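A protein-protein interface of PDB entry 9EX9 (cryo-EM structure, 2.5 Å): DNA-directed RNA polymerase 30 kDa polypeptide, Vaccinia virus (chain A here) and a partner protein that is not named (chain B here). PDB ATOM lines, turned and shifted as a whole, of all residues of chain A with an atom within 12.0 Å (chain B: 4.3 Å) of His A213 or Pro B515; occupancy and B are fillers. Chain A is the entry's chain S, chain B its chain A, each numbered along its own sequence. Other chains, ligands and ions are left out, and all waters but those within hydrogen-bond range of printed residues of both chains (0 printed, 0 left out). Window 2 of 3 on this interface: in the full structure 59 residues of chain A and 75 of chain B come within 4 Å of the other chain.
The backbone carbonyl oxygen (O) of Pro B515 lies within hydrogen-bond range of a ring nitrogen (NE2) of His A213, 3.1 Å away.
The backbone carbonyl oxygen (O) of His A213 lies close to the side-chain amide oxygen (OD1) of Asn A215.
O of His A213 touches CD2 of His B538 (3.7 Å). CD2 of His A213 touches CD2 of Leu B539, 3.99 Å away. Lys A216 touches Tyr B514 (NZ to OH, 3.9 Å). His B538 touches Lys A216. His B538 touches Glu A217.
Of the printed residues of chain B, His A213 touches Pro B515 (3.1 Å), His B538 (3.7 Å) and Leu B539 (3.99 Å). Of the printed residues of chain A, Pro B515 touches His A213 (3.1 Å). Of the printed residues of chain A, Tyr B514 touches Lys A216 (3.9 Å). No residue of chain A comes within 4 Å of Gly B516. No residue of chain A comes within 4 Å of Leu B517. His B538 touches just these residues of chain A: His A213 (3.7 Å), Lys A216 (3.4 Å) and Glu A217 (3.8 Å). Of the printed residues of chain B, Lys A216 touches Tyr B514 (3.9 Å) and His B538 (3.4 Å). Of the printed residues of chain B, Glu A217 touches His B538 (3.8 Å). Glu A214 touches none of the printed residues of chain B.
Hydrophobic or aromatic side chains of chain B that line the printed part of chain A: Tyr B514, His B538 and Leu B539. Of the 11 printed residues of chain A, 3 touch a printed residue of chain B. Hydrophobic or aromatic side chains of chain A that line the printed part of chain B: His A213. Among the printed residues, no Asp or Glu carboxylate lies within 4 Å of a Lys or Arg side-chain nitrogen of the other chain.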
ATOM      1  N   THR A 209      25.044  -7.789  12.937  1.00  0.00           N
ATOM      2  CA  THR A 209      24.347  -9.045  13.154  1.00  0.00           C
ATOM      3  C   THR A 209      24.071  -9.735  11.819  1.00  0.00           C
ATOM      4  O   THR A 209      24.383  -9.221  10.741  1.00  0.00           O
ATOM      5  CB  THR A 209      23.037  -8.820  13.909  1.00  0.00           C
ATOM      6  OG1 THR A 209      22.177  -7.967  13.144  1.00  0.00           O
ATOM      7  CG2 THR A 209      23.305  -8.188  15.262  1.00  0.00           C
ATOM      8  N   GLN A 210      23.479 -10.917  11.906  1.00  0.00           N
ATOM      9  CA  GLN A 210      23.205 -11.733  10.735  1.00  0.00           C
ATOM     10  C   GLN A 210      21.739 -11.626  10.329  1.00  0.00           C
ATOM     11  O   GLN A 210      20.882 -11.192  11.102  1.00  0.00           O
ATOM     12  CB  GLN A 210      23.578 -13.191  11.002  1.00  0.00           C
ATOM     13  CG  GLN A 210      23.046 -13.756  12.307  1.00  0.00           C
ATOM     14  CD  GLN A 210      23.520 -15.169  12.558  1.00  0.00           C
ATOM     15  OE1 GLN A 210      24.108 -15.801  11.682  1.00  0.00           O
ATOM     16  NE2 GLN A 210      23.272 -15.672  13.759  1.00  0.00           N
ATOM     17  N   SER A 211      21.463 -12.024   9.090  1.00  0.00           N
ATOM     18  CA  SER A 211      20.125 -11.982   8.517  1.00  0.00           C
ATOM     19  C   SER A 211      19.726 -13.382   8.076  1.00  0.00           C
ATOM     20  O   SER A 211      20.475 -14.042   7.349  1.00  0.00           O
ATOM     21  CB  SER A 211      20.069 -11.020   7.329  1.00  0.00           C
ATOM     22  OG  SER A 211      20.512  -9.728   7.701  1.00  0.00           O
ATOM     23  N   ILE A 212      18.549 -13.828   8.508  1.00  0.00           N
ATOM     24  CA  ILE A 212      18.058 -15.157   8.165  1.00  0.00           C
ATOM     25  C   ILE A 212      16.721 -15.019   7.445  1.00  0.00           C
ATOM     26  O   ILE A 212      16.571 -15.470   6.304  1.00  0.00           O
ATOM     27  CB  ILE A 212      17.939 -16.054   9.415  1.00  0.00           C
ATOM     28  CG1 ILE A 212      19.311 -16.287  10.056  1.00  0.00           C
ATOM     29  CG2 ILE A 212      17.346 -17.412   9.061  1.00  0.00           C
ATOM     30  CD1 ILE A 212      19.852 -15.116  10.824  1.00  0.00           C
ATOM     31  N   HIS A 213      15.746 -14.394   8.099  1.00  0.00           N
ATOM     32  CA  HIS A 213      14.397 -14.227   7.563  1.00  0.00           C
ATOM     33  C   HIS A 213      13.986 -12.761   7.609  1.00  0.00           C
ATOM     34  O   HIS A 213      12.879 -12.411   8.021  1.00  0.00           O
ATOM     35  CB  HIS A 213      13.404 -15.091   8.334  1.00  0.00           C
ATOM     36  CG  HIS A 213      13.472 -16.544   7.991  1.00  0.00           C
ATOM     37  ND1 HIS A 213      12.891 -17.069   6.857  1.00  0.00           N
ATOM     38  CD2 HIS A 213      14.046 -17.587   8.635  1.00  0.00           C
ATOM     39  CE1 HIS A 213      13.108 -18.371   6.816  1.00  0.00           C
ATOM     40  NE2 HIS A 213      13.806 -18.711   7.884  1.00  0.00           N
ATOM     41  N   GLU A 214      14.881 -11.881   7.149  1.00  0.00           N
ATOM     42  CA  GLU A 214      14.706 -10.447   7.356  1.00  0.00           C
ATOM     43  C   GLU A 214      13.346  -9.953   6.882  1.00  0.00           C
ATOM     44  O   GLU A 214      12.843  -8.944   7.387  1.00  0.00           O
ATOM     45  CB  GLU A 214      15.815  -9.679   6.635  1.00  0.00           C
ATOM     46  CG  GLU A 214      15.751  -8.171   6.816  1.00  0.00           C
ATOM     47  CD  GLU A 214      16.744  -7.439   5.937  1.00  0.00           C
ATOM     48  OE1 GLU A 214      17.597  -8.109   5.319  1.00  0.00           O
ATOM     49  OE2 GLU A 214      16.668  -6.196   5.860  1.00  0.00           O
ATOM     50  N   ASN A 215      12.736 -10.641   5.921  1.00  0.00           N
ATOM     51  CA  ASN A 215      11.440 -10.208   5.409  1.00  0.00           C
ATOM     52  C   ASN A 215      10.311 -10.388   6.417  1.00  0.00           C
ATOM     53  O   ASN A 215       9.199  -9.918   6.155  1.00  0.00           O
ATOM     54  CB  ASN A 215      11.107 -10.951   4.113  1.00  0.00           C
ATOM     55  CG  ASN A 215      11.476 -12.417   4.167  1.00  0.00           C
ATOM     56  OD1 ASN A 215      11.765 -12.954   5.234  1.00  0.00           O
ATOM     57  ND2 ASN A 215      11.464 -13.073   3.014  1.00  0.00           N
ATOM     58  N   LYS A 216      10.556 -11.054   7.550  1.00  0.00           N
ATOM     59  CA  LYS A 216       9.556 -11.204   8.603  1.00  0.00           C
ATOM     60  C   LYS A 216      10.010 -10.601   9.929  1.00  0.00           C
ATOM     61  O   LYS A 216       9.454 -10.937  10.977  1.00  0.00           O
ATOM     62  CB  LYS A 216       9.200 -12.678   8.801  1.00  0.00           C
ATOM     63  CG  LYS A 216       8.453 -13.286   7.633  1.00  0.00           C
ATOM     64  CD  LYS A 216       8.156 -14.758   7.849  1.00  0.00           C
ATOM     65  CE  LYS A 216       9.426 -15.582   7.890  1.00  0.00           C
ATOM     66  NZ  LYS A 216       9.142 -17.038   7.817  1.00  0.00           N
ATOM     67  N   GLU A 217      10.998  -9.714   9.908  1.00  0.00           N
ATOM     68  CA  GLU A 217      11.516  -9.146  11.144  1.00  0.00           C
ATOM     69  C   GLU A 217      10.477  -8.252  11.816  1.00  0.00           C
ATOM     70  O   GLU A 217       9.615  -7.661  11.163  1.00  0.00           O
ATOM     71  CB  GLU A 217      12.790  -8.352  10.866  1.00  0.00           C
ATOM     72  CG  GLU A 217      13.467  -7.818  12.112  1.00  0.00           C
ATOM     73  CD  GLU A 217      14.849  -7.273  11.832  1.00  0.00           C
ATOM     74  OE1 GLU A 217      15.201  -7.129  10.644  1.00  0.00           O
ATOM     75  OE2 GLU A 217      15.585  -6.991  12.799  1.00  0.00           O
ATOM     76  N   ILE A 218      10.569  -8.161  13.142  1.00  0.00           N
ATOM     77  CA  ILE A 218       9.673  -7.349  13.958  1.00  0.00           C
ATOM     78  C   ILE A 218      10.516  -6.333  14.718  1.00  0.00           C
ATOM     79  O   ILE A 218      11.499  -6.701  15.371  1.00  0.00           O
ATOM     80  CB  ILE A 218       8.848  -8.212  14.931  1.00  0.00           C
ATOM     81  CG1 ILE A 218       8.089  -9.298  14.168  1.00  0.00           C
ATOM     82  CG2 ILE A 218       7.871  -7.348  15.713  1.00  0.00           C
ATOM     83  CD1 ILE A 218       7.387 -10.290  15.063  1.00  0.00           C
ATOM     84  N   THR A 219      10.124  -5.063  14.643  1.00  0.00           N
ATOM     85  CA  THR A 219      10.901  -3.972  15.219  1.00  0.00           C
ATOM     86  C   THR A 219      10.440  -3.667  16.640  1.00  0.00           C
ATOM     87  O   THR A 219       9.253  -3.771  16.957  1.00  0.00           O
ATOM     88  CB  THR A 219      10.781  -2.714  14.359  1.00  0.00           C
ATOM     89  OG1 THR A 219      11.018  -3.043  12.985  1.00  0.00           O
ATOM     90  CG2 THR A 219      11.789  -1.668  14.804  1.00  0.00           C
ATOM     91  N   TYR B 514      14.019 -26.409  10.958  1.00  0.00           N
ATOM     92  CA  TYR B 514      13.399 -25.167  10.574  1.00  0.00           C
ATOM     93  C   TYR B 514      14.380 -24.480   9.636  1.00  0.00           C
ATOM     94  O   TYR B 514      15.540 -24.285  10.023  1.00  0.00           O
ATOM     95  CB  TYR B 514      13.084 -24.268  11.766  1.00  0.00           C
ATOM     96  CG  TYR B 514      12.232 -23.075  11.406  1.00  0.00           C
ATOM     97  CD1 TYR B 514      10.903 -23.232  11.054  1.00  0.00           C
ATOM     98  CD2 TYR B 514      12.756 -21.795  11.420  1.00  0.00           C
ATOM     99  CE1 TYR B 514      10.128 -22.151  10.721  1.00  0.00           C
ATOM    100  CE2 TYR B 514      11.985 -20.708  11.090  1.00  0.00           C
ATOM    101  CZ  TYR B 514      10.673 -20.892  10.741  1.00  0.00           C
ATOM    102  OH  TYR B 514       9.895 -19.811  10.411  1.00  0.00           O
ATOM    103  N   PRO B 515      13.965 -24.105   8.427  1.00  0.00           N
ATOM    104  CA  PRO B 515      14.929 -23.567   7.459  1.00  0.00           C
ATOM    105  C   PRO B 515      15.671 -22.373   8.034  1.00  0.00           C
ATOM    106  O   PRO B 515      15.064 -21.437   8.554  1.00  0.00           O
ATOM    107  CB  PRO B 515      14.053 -23.175   6.265  1.00  0.00           C
ATOM    108  CG  PRO B 515      12.690 -23.032   6.815  1.00  0.00           C
ATOM    109  CD  PRO B 515      12.586 -24.022   7.923  1.00  0.00           C
ATOM    110  N   GLY B 516      16.993 -22.400   7.917  1.00  0.00           N
ATOM    111  CA  GLY B 516      17.799 -21.435   8.631  1.00  0.00           C
ATOM    112  C   GLY B 516      18.305 -21.983   9.948  1.00  0.00           C
ATOM    113  O   GLY B 516      19.367 -22.603  10.003  1.00  0.00           O
ATOM    114  N   LEU B 517      17.554 -21.745  11.021  1.00  0.00           N
ATOM    115  CA  LEU B 517      18.074 -21.942  12.370  1.00  0.00           C
ATOM    116  C   LEU B 517      18.542 -23.374  12.606  1.00  0.00           C
ATOM    117  O   LEU B 517      19.729 -23.618  12.839  1.00  0.00           O
ATOM    118  CB  LEU B 517      17.008 -21.565  13.394  1.00  0.00           C
ATOM    119  CG  LEU B 517      16.664 -20.086  13.526  1.00  0.00           C
ATOM    120  CD1 LEU B 517      15.858 -19.603  12.344  1.00  0.00           C
ATOM    121  CD2 LEU B 517      15.907 -19.862  14.816  1.00  0.00           C
ATOM    122  N   HIS B 538      11.480 -12.656  15.829  1.00  0.00           N
ATOM    123  CA  HIS B 538      10.918 -13.563  14.839  1.00  0.00           C
ATOM    124  C   HIS B 538      11.699 -14.861  14.689  1.00  0.00           C
ATOM    125  O   HIS B 538      11.322 -15.696  13.862  1.00  0.00           O
ATOM    126  CB  HIS B 538      10.826 -12.862  13.478  1.00  0.00           C
ATOM    127  CG  HIS B 538      12.155 -12.538  12.868  1.00  0.00           C
ATOM    128  ND1 HIS B 538      13.073 -11.708  13.473  1.00  0.00           N
ATOM    129  CD2 HIS B 538      12.715 -12.927  11.699  1.00  0.00           C
ATOM    130  CE1 HIS B 538      14.144 -11.606  12.707  1.00  0.00           C
ATOM    131  NE2 HIS B 538      13.952 -12.336  11.624  1.00  0.00           N
ATOM    132  N   LEU B 539      12.765 -15.064  15.462  1.00  0.00           N
ATOM    133  CA  LEU B 539      13.569 -16.276  15.366  1.00  0.00           C
ATOM    134  C   LEU B 539      13.700 -16.987  16.708  1.00  0.00           C
ATOM    135  O   LEU B 539      14.579 -17.836  16.870  1.00  0.00           O
ATOM    136  CB  LEU B 539      14.957 -15.952  14.807  1.00  0.00           C
ATOM    137  CG  LEU B 539      15.039 -15.276  13.436  1.00  0.00           C
ATOM    138  CD1 LEU B 539      16.480 -14.912  13.135  1.00  0.00           C
ATOM    139  CD2 LEU B 539      14.479 -16.149  12.327  1.00  0.00           C
